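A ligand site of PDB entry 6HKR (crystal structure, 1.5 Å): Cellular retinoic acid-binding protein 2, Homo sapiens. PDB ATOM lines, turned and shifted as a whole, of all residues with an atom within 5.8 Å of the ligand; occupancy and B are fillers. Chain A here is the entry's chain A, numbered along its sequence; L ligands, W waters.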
ATOM      1  N   ILE A  10      32.259 -32.594   0.182  1.00  0.00           N
ATOM      2  CA  ILE A  10      33.180 -32.441  -0.920  1.00  0.00           C
ATOM      3  C   ILE A  10      34.616 -32.831  -0.522  1.00  0.00           C
ATOM      4  O   ILE A  10      35.122 -32.481   0.571  1.00  0.00           O
ATOM      5  CB  ILE A  10      33.137 -30.995  -1.479  1.00  0.00           C
ATOM      6  CG1 ILE A  10      33.759 -30.919  -2.880  1.00  0.00           C
ATOM      7  CG2 ILE A  10      33.705 -29.985  -0.489  1.00  0.00           C
ATOM      8  CD1 ILE A  10      33.301 -29.701  -3.639  1.00  0.00           C
ATOM      9  N   PHE A  16      35.968 -24.667 -11.031  1.00  0.00           N
ATOM     10  CA  PHE A  16      34.766 -23.888 -10.708  1.00  0.00           C
ATOM     11  C   PHE A  16      34.897 -22.428 -11.127  1.00  0.00           C
ATOM     12  O   PHE A  16      33.984 -21.876 -11.719  1.00  0.00           O
ATOM     13  CB  PHE A  16      34.415 -24.047  -9.226  1.00  0.00           C
ATOM     14  CG  PHE A  16      33.113 -23.414  -8.834  1.00  0.00           C
ATOM     15  CD1 PHE A  16      31.950 -23.671  -9.552  1.00  0.00           C
ATOM     16  CD2 PHE A  16      33.046 -22.492  -7.815  1.00  0.00           C
ATOM     17  CE1 PHE A  16      30.733 -23.113  -9.178  1.00  0.00           C
ATOM     18  CE2 PHE A  16      31.832 -21.903  -7.453  1.00  0.00           C
ATOM     19  CZ  PHE A  16      30.680 -22.228  -8.132  1.00  0.00           C
ATOM     20  N   LEU A  20      32.455 -20.206 -13.888  1.00  0.00           N
ATOM     21  CA  LEU A  20      31.807 -18.921 -13.654  1.00  0.00           C
ATOM     22  C   LEU A  20      32.301 -17.842 -14.628  1.00  0.00           C
ATOM     23  O   LEU A  20      31.493 -16.972 -15.054  1.00  0.00           O
ATOM     24  CB  LEU A  20      32.040 -18.512 -12.208  1.00  0.00           C
ATOM     25  CG  LEU A  20      31.457 -19.416 -11.153  1.00  0.00           C
ATOM     26  CD1 LEU A  20      31.685 -18.802  -9.769  1.00  0.00           C
ATOM     27  CD2 LEU A  20      29.989 -19.689 -11.371  1.00  0.00           C
ATOM     28  N   VAL A  25      30.397 -14.179 -15.052  1.00  0.00           N
ATOM     29  CA  VAL A  25      30.363 -13.664 -13.688  1.00  0.00           C
ATOM     30  C   VAL A  25      31.642 -12.813 -13.458  1.00  0.00           C
ATOM     31  O   VAL A  25      32.755 -13.271 -13.743  1.00  0.00           O
ATOM     32  CB  VAL A  25      30.236 -14.820 -12.680  1.00  0.00           C
ATOM     33  CG1 VAL A  25      30.182 -14.286 -11.233  1.00  0.00           C
ATOM     34  CG2 VAL A  25      29.032 -15.721 -12.979  1.00  0.00           C
ATOM     35  N   MET A  28      34.911 -10.024  -8.847  1.00  0.00           N
ATOM     36  CA  MET A  28      34.614  -9.937  -7.416  1.00  0.00           C
ATOM     37  C   MET A  28      33.482 -10.886  -7.011  1.00  0.00           C
ATOM     38  O   MET A  28      33.595 -11.581  -5.986  1.00  0.00           O
ATOM     39  CB  MET A  28      34.421  -8.484  -6.973  1.00  0.00           C
ATOM     40  CG  MET A  28      35.841  -7.869  -6.963  1.00  0.00           C
ATOM     41  SD  MET A  28      36.012  -6.140  -6.921  1.00  0.00           S
ATOM     42  CE  MET A  28      35.644  -5.601  -8.579  1.00  0.00           C
ATOM     43  N   LEU A  29      32.449 -11.027  -7.828  1.00  0.00           N
ATOM     44  CA  LEU A  29      31.420 -12.039  -7.476  1.00  0.00           C
ATOM     45  C   LEU A  29      31.978 -13.469  -7.554  1.00  0.00           C
ATOM     46  O   LEU A  29      31.589 -14.323  -6.732  1.00  0.00           O
ATOM     47  CB  LEU A  29      30.234 -11.892  -8.427  1.00  0.00           C
ATOM     48  CG  LEU A  29      29.409 -10.617  -8.297  1.00  0.00           C
ATOM     49  CD1 LEU A  29      28.254 -10.620  -9.293  1.00  0.00           C
ATOM     50  CD2 LEU A  29      28.870 -10.419  -6.892  1.00  0.00           C
ATOM     51  N   ILE A  32      33.814 -14.372  -4.326  1.00  0.00           N
ATOM     52  CA  ILE A  32      32.851 -14.712  -3.262  1.00  0.00           C
ATOM     53  C   ILE A  32      32.316 -16.142  -3.440  1.00  0.00           C
ATOM     54  O   ILE A  32      32.251 -16.915  -2.472  1.00  0.00           O
ATOM     55  CB  ILE A  32      31.691 -13.700  -3.250  1.00  0.00           C
ATOM     56  CG1 ILE A  32      32.202 -12.290  -2.965  1.00  0.00           C
ATOM     57  CG2 ILE A  32      30.668 -14.156  -2.235  1.00  0.00           C
ATOM     58  CD1 ILE A  32      31.186 -11.163  -3.167  1.00  0.00           C
ATOM     59  N   ALA A  33      31.863 -16.468  -4.646  1.00  0.00           N
ATOM     60  CA  ALA A  33      31.239 -17.741  -4.930  1.00  0.00           C
ATOM     61  C   ALA A  33      32.234 -18.883  -4.739  1.00  0.00           C
ATOM     62  O   ALA A  33      31.847 -19.882  -4.202  1.00  0.00           O
ATOM     63  CB  ALA A  33      30.696 -17.732  -6.331  1.00  0.00           C
ATOM     64  N   ALA A  36      32.851 -19.548  -1.062  1.00  0.00           N
ATOM     65  CA  ALA A  36      31.732 -20.114  -0.376  1.00  0.00           C
ATOM     66  C   ALA A  36      31.500 -21.564  -0.819  1.00  0.00           C
ATOM     67  O   ALA A  36      31.129 -22.431   0.004  1.00  0.00           O
ATOM     68  CB  ALA A  36      30.525 -19.224  -0.573  1.00  0.00           C
ATOM     69  N   ALA A  37      31.718 -21.845  -2.102  1.00  0.00           N
ATOM     70  CA  ALA A  37      31.519 -23.171  -2.690  1.00  0.00           C
ATOM     71  C   ALA A  37      32.578 -24.180  -2.232  1.00  0.00           C
ATOM     72  O   ALA A  37      32.424 -25.385  -2.447  1.00  0.00           O
ATOM     73  CB  ALA A  37      31.500 -23.088  -4.184  1.00  0.00           C
ATOM     74  N   PRO A  40      30.524 -26.575   0.845  1.00  0.00           N
ATOM     75  CA  PRO A  40      29.065 -26.619   0.790  1.00  0.00           C
ATOM     76  C   PRO A  40      28.497 -27.740   1.656  1.00  0.00           C
ATOM     77  O   PRO A  40      29.218 -28.670   2.004  1.00  0.00           O
ATOM     78  CB  PRO A  40      28.824 -27.000  -0.662  1.00  0.00           C
ATOM     79  CG  PRO A  40      29.961 -27.895  -0.973  1.00  0.00           C
ATOM     80  CD  PRO A  40      31.149 -27.336  -0.240  1.00  0.00           C
ATOM     81  N   VAL A  42      25.514 -30.528   1.160  1.00  0.00           N
ATOM     82  CA  VAL A  42      24.724 -31.134   0.092  1.00  0.00           C
ATOM     83  C   VAL A  42      23.862 -32.249   0.691  1.00  0.00           C
ATOM     84  O   VAL A  42      24.414 -33.217   1.247  1.00  0.00           O
ATOM     85  CB  VAL A  42      25.616 -31.683  -1.032  1.00  0.00           C
ATOM     86  CG1 VAL A  42      24.755 -32.414  -2.059  1.00  0.00           C
ATOM     87  CG2 VAL A  42      26.425 -30.568  -1.693  1.00  0.00           C
ATOM     88  N   THR A  55      21.636 -27.736  -1.949  1.00  0.00           N
ATOM     89  CA  THR A  55      23.042 -27.373  -1.936  1.00  0.00           C
ATOM     90  C   THR A  55      23.147 -26.010  -1.243  1.00  0.00           C
ATOM     91  O   THR A  55      22.617 -25.057  -1.765  1.00  0.00           O
ATOM     92  CB  THR A  55      23.631 -27.338  -3.331  1.00  0.00           C
ATOM     93  OG1 THR A  55      23.452 -28.626  -3.918  1.00  0.00           O
ATOM     94  CG2 THR A  55      25.103 -27.003  -3.312  1.00  0.00           C
ATOM     95  N   THR A  57      25.336 -22.986   0.953  1.00  0.00           N
ATOM     96  CA  THR A  57      26.525 -22.231   1.339  1.00  0.00           C
ATOM     97  C   THR A  57      26.094 -21.018   2.165  1.00  0.00           C
ATOM     98  O   THR A  57      24.889 -20.713   2.281  1.00  0.00           O
ATOM     99  CB  THR A  57      27.339 -21.759   0.134  1.00  0.00           C
ATOM    100  OG1 THR A  57      26.691 -20.653  -0.488  1.00  0.00           O
ATOM    101  CG2 THR A  57      27.649 -22.863  -0.850  1.00  0.00           C
ATOM    102  N   VAL A  59      26.250 -18.022   1.382  1.00  0.00           N
ATOM    103  CA  VAL A  59      25.864 -16.892   0.508  1.00  0.00           C
ATOM    104  C   VAL A  59      24.732 -17.260  -0.453  1.00  0.00           C
ATOM    105  O   VAL A  59      24.232 -16.361  -1.135  1.00  0.00           O
ATOM    106  CB  VAL A  59      27.085 -16.350  -0.263  1.00  0.00           C
ATOM    107  CG1 VAL A  59      28.077 -15.697   0.684  1.00  0.00           C
ATOM    108  CG2 VAL A  59      27.785 -17.387  -1.119  1.00  0.00           C
ATOM    109  N   ARG A  60      24.394 -18.551  -0.583  1.00  0.00           N
ATOM    110  CA  ARG A  60      23.428 -18.984  -1.564  1.00  0.00           C
ATOM    111  C   ARG A  60      23.093 -20.439  -1.290  1.00  0.00           C
ATOM    112  O   ARG A  60      23.995 -21.256  -1.095  1.00  0.00           O
ATOM    113  CB  ARG A  60      23.990 -18.828  -2.986  1.00  0.00           C
ATOM    114  CG  ARG A  60      23.068 -19.293  -4.111  1.00  0.00           C
ATOM    115  CD  ARG A  60      23.623 -18.933  -5.501  1.00  0.00           C
ATOM    116  NE  ARG A  60      23.066 -19.714  -6.632  1.00  0.00           N
ATOM    117  CZ  ARG A  60      21.923 -19.457  -7.244  1.00  0.00           C
ATOM    118  NH1 ARG A  60      21.186 -18.399  -6.903  1.00  0.00           N
ATOM    119  NH2 ARG A  60      21.504 -20.289  -8.202  1.00  0.00           N
ATOM    120  N   VAL A  77      23.859 -22.237 -12.882  1.00  0.00           N
ATOM    121  CA  VAL A  77      24.811 -22.087 -11.783  1.00  0.00           C
ATOM    122  C   VAL A  77      25.043 -20.589 -11.479  1.00  0.00           C
ATOM    123  O   VAL A  77      25.307 -20.241 -10.345  1.00  0.00           O
ATOM    124  CB  VAL A  77      26.110 -22.905 -12.037  1.00  0.00           C
ATOM    125  CG1 VAL A  77      26.842 -22.470 -13.251  1.00  0.00           C
ATOM    126  CG2 VAL A  77      27.048 -22.865 -10.850  1.00  0.00           C
ATOM    127  N   ASP A  78      24.873 -19.718 -12.466  1.00  0.00           N
ATOM    128  CA  ASP A  78      25.033 -18.275 -12.272  1.00  0.00           C
ATOM    129  C   ASP A  78      23.719 -17.561 -11.917  1.00  0.00           C
ATOM    130  O   ASP A  78      23.651 -16.362 -11.907  1.00  0.00           O
ATOM    131  CB  ASP A  78      25.741 -17.680 -13.468  1.00  0.00           C
ATOM    132  CG  ASP A  78      24.968 -17.736 -14.743  1.00  0.00           C
ATOM    133  OD1 ASP A  78      24.516 -18.867 -15.116  1.00  0.00           O
ATOM    134  OD2 ASP A  78      24.851 -16.692 -15.372  1.00  0.00           O
ATOM    135  N   GLY A  79      22.669 -18.319 -11.628  1.00  0.00           N
ATOM    136  CA  GLY A  79      21.434 -17.729 -11.067  1.00  0.00           C
ATOM    137  C   GLY A  79      20.321 -17.404 -12.082  1.00  0.00           C
ATOM    138  O   GLY A  79      19.315 -16.791 -11.729  1.00  0.00           O
ATOM    139  N   ARG A 112      25.281 -35.940 -12.531  1.00  0.00           N
ATOM    140  CA  ARG A 112      25.649 -36.547 -11.225  1.00  0.00           C
ATOM    141  C   ARG A 112      25.811 -38.061 -11.417  1.00  0.00           C
ATOM    142  O   ARG A 112      24.928 -38.676 -12.031  1.00  0.00           O
ATOM    143  CB  ARG A 112      24.633 -36.239 -10.126  1.00  0.00           C
ATOM    144  CG  ARG A 112      24.747 -34.822  -9.612  1.00  0.00           C
ATOM    145  CD  ARG A 112      23.811 -34.465  -8.478  1.00  0.00           C
ATOM    146  NE  ARG A 112      24.102 -33.210  -7.783  1.00  0.00           N
ATOM    147  CZ  ARG A 112      23.570 -32.021  -8.077  1.00  0.00           C
ATOM    148  NH1 ARG A 112      22.651 -31.907  -9.050  1.00  0.00           N
ATOM    149  NH2 ARG A 112      23.940 -30.957  -7.387  1.00  0.00           N
ATOM    150  N   LEU A 122      29.794 -34.676  -9.337  1.00  0.00           N
ATOM    151  CA  LEU A 122      28.986 -33.676 -10.018  1.00  0.00           C
ATOM    152  C   LEU A 122      29.859 -33.031 -11.091  1.00  0.00           C
ATOM    153  O   LEU A 122      30.991 -32.660 -10.796  1.00  0.00           O
ATOM    154  CB  LEU A 122      28.556 -32.600  -9.020  1.00  0.00           C
ATOM    155  CG  LEU A 122      27.982 -31.290  -9.601  1.00  0.00           C
ATOM    156  CD1 LEU A 122      26.589 -31.499 -10.190  1.00  0.00           C
ATOM    157  CD2 LEU A 122      27.901 -30.242  -8.500  1.00  0.00           C
ATOM    158  N   MET A 124      29.429 -29.721 -13.849  1.00  0.00           N
ATOM    159  CA  MET A 124      28.688 -28.592 -14.369  1.00  0.00           C
ATOM    160  C   MET A 124      29.446 -28.067 -15.597  1.00  0.00           C
ATOM    161  O   MET A 124      30.630 -27.863 -15.525  1.00  0.00           O
ATOM    162  CB  MET A 124      28.543 -27.504 -13.310  1.00  0.00           C
ATOM    163  CG  MET A 124      27.790 -27.979 -12.072  1.00  0.00           C
ATOM    164  SD  MET A 124      27.757 -26.717 -10.749  1.00  0.00           S
ATOM    165  CE  MET A 124      29.436 -26.733 -10.162  1.00  0.00           C
ATOM    166  N   ARG A 133      33.334 -31.977  -9.449  1.00  0.00           N
ATOM    167  CA  ARG A 133      33.359 -31.987  -7.980  1.00  0.00           C
ATOM    168  C   ARG A 133      33.054 -33.394  -7.490  1.00  0.00           C
ATOM    169  O   ARG A 133      32.189 -34.078  -8.024  1.00  0.00           O
ATOM    170  CB  ARG A 133      32.368 -30.947  -7.428  1.00  0.00           C
ATOM    171  CG  ARG A 133      32.783 -29.560  -7.879  1.00  0.00           C
ATOM    172  CD  ARG A 133      31.851 -28.432  -7.594  1.00  0.00           C
ATOM    173  NE  ARG A 133      31.434 -28.267  -6.229  1.00  0.00           N
ATOM    174  CZ  ARG A 133      31.896 -27.290  -5.410  1.00  0.00           C
ATOM    175  NH1 ARG A 133      32.988 -26.606  -5.691  1.00  0.00           N
ATOM    176  NH2 ARG A 133      31.230 -27.035  -4.312  1.00  0.00           N
ATOM    177  N   TYR A 135      32.502 -36.028  -4.099  1.00  0.00           N
ATOM    178  CA  TYR A 135      31.963 -36.020  -2.733  1.00  0.00           C
ATOM    179  C   TYR A 135      31.959 -37.455  -2.192  1.00  0.00           C
ATOM    180  O   TYR A 135      31.844 -38.449  -2.952  1.00  0.00           O
ATOM    181  CB  TYR A 135      30.512 -35.501  -2.675  1.00  0.00           C
ATOM    182  CG  TYR A 135      30.276 -34.173  -3.354  1.00  0.00           C
ATOM    183  CD1 TYR A 135      30.164 -34.124  -4.734  1.00  0.00           C
ATOM    184  CD2 TYR A 135      30.074 -33.011  -2.633  1.00  0.00           C
ATOM    185  CE1 TYR A 135      29.931 -32.921  -5.372  1.00  0.00           C
ATOM    186  CE2 TYR A 135      29.783 -31.815  -3.258  1.00  0.00           C
ATOM    187  CZ  TYR A 135      29.742 -31.765  -4.646  1.00  0.00           C
ATOM    188  OH  TYR A 135      29.503 -30.595  -5.316  1.00  0.00           O
HETATM  189  C1  LIG L   1      27.209 -16.781  -5.828  1.00  0.00           C
HETATM  190  C2  LIG L   1      28.186 -25.489  -4.390  1.00  0.00           C
HETATM  191  C3  LIG L   1      27.033 -17.485  -7.023  1.00  0.00           C
HETATM  192  C4  LIG L   1      27.553 -17.490  -4.673  1.00  0.00           C
HETATM  193  C5  LIG L   1      27.710 -22.134  -5.893  1.00  0.00           C
HETATM  194  C6  LIG L   1      27.634 -18.865  -4.696  1.00  0.00           C
HETATM  195  C7  LIG L   1      27.421 -19.561  -5.869  1.00  0.00           C
HETATM  196  C8  LIG L   1      27.153 -18.850  -7.022  1.00  0.00           C
HETATM  197  C9  LIG L   1      27.557 -20.992  -5.914  1.00  0.00           C
HETATM  198  C10 LIG L   1      27.820 -23.562  -5.771  1.00  0.00           C
HETATM  199  C11 LIG L   1      28.119 -24.126  -4.540  1.00  0.00           C
HETATM  200  N1  LIG L   1      27.133 -15.406  -5.796  1.00  0.00           N
HETATM  201  C12 LIG L   1      26.566 -14.695  -6.933  1.00  0.00           C
HETATM  202  C13 LIG L   1      26.692 -16.789  -8.343  1.00  0.00           C
HETATM  203  C14 LIG L   1      27.009 -15.294  -8.207  1.00  0.00           C
HETATM  204  C15 LIG L   1      27.933 -26.321  -5.459  1.00  0.00           C
HETATM  205  C16 LIG L   1      27.582 -25.770  -6.683  1.00  0.00           C
HETATM  206  C17 LIG L   1      27.520 -24.399  -6.836  1.00  0.00           C
HETATM  207  C18 LIG L   1      27.958 -27.820  -5.276  1.00  0.00           C
HETATM  208  O1  LIG L   1      27.104 -28.490  -5.956  1.00  0.00           O
HETATM  209  O2  LIG L   1      28.726 -28.299  -4.407  1.00  0.00           O
HETATM  210  C19 LIG L   1      27.544 -14.643  -4.566  1.00  0.00           C
HETATM  211  C20 LIG L   1      28.215 -13.353  -4.894  1.00  0.00           C
HETATM  212  C21 LIG L   1      26.377 -14.429  -3.646  1.00  0.00           C
HETATM  213  C22 LIG L   1      25.202 -16.989  -8.675  1.00  0.00           C
HETATM  214  C23 LIG L   1      27.512 -17.325  -9.528  1.00  0.00           C
HETATM  215  O   HOH W   1      24.765 -27.639  -7.036  1.00  0.00           O
HETATM  216  O   HOH W   2      25.573 -30.441  -5.078  1.00  0.00           O
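O2 of the ligand is in hydrogen-bond range of OH of Tyr 135. An oxygen (O2) of the ligand is in salt-bridge range of the guanidinium group (NH2) of Arg 133, 2.8 Å away.
The guanidinium group of Arg 133 is in hydrogen-bond range of the side-chain hydroxyl of Tyr 135 (3.2 Å). The backbone NH (N) of Arg 133 is in hydrogen-bond range of the backbone carbonyl oxygen (O) of Leu 122 (2.8 Å). O of Ala 37 is in hydrogen-bond range of NH2 of Arg 133 (2.8 Å). The side-chain hydroxyl of Thr 57 lies close to the backbone NH of Val 59, at 3.3 Å. The backbone carbonyl oxygen (O) of Arg 60 is in hydrogen-bond range of the side-chain hydroxyl (OG1) of Thr 57 (2.8 Å). O of Leu 20 lies within hydrogen-bond range of N of Val 25 (3.0 Å).
Phe 16 touches the ligand. Leu 20 touches the ligand (CD2 to C23, 3.9 Å). CD2 of Leu 29 touches C20 of the ligand (3.6 Å). CG2 of Ile 32 touches C20 of the ligand, 3.7 Å away. CB of Ala 33 touches C4 of the ligand, 3.6 Å away. Ala 37 touches the ligand. Pro 40 touches the ligand (CG to O2, 3.7 Å). Thr 55 touches the ligand (CG2 to C18, 3.6 Å). Thr 57 touches the ligand. CG2 of Val 59 touches C4 of the ligand, at 3.6 Å. Arg 60 touches the ligand (CD to C8, 3.8 Å). Val 77 touches the ligand. Asp 78 touches the ligand. Leu 122 touches the ligand. Hydrophobic or aromatic side chains within 4 Å of the ligand: Phe 16, Leu 20, Leu 29, Ile 32, Ala 33, Ala 37, Pro 40, Val 59, Leu 122 and Tyr 135. 16 residues have an atom within 4 Å of the ligand: Phe 16, Leu 20, Leu 29, Ile 32, Ala 33, Ala 37, Pro 40, Thr 55, Thr 57, Val 59, Arg 60, Val 77, Asp 78, Leu 122, Arg 133 and Tyr 135. The nearest printed residue that does not touch the ligand is Met 124 (4.1 Å).
Water W2 lies within hydrogen-bond range of O1 of the ligand, NH2 of Arg 112 and OG1 of Thr 55. Water W1 lies within hydrogen-bond range of O1 of the ligand (2.7 Å) and NH2 of Arg 112 (3.4 Å).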
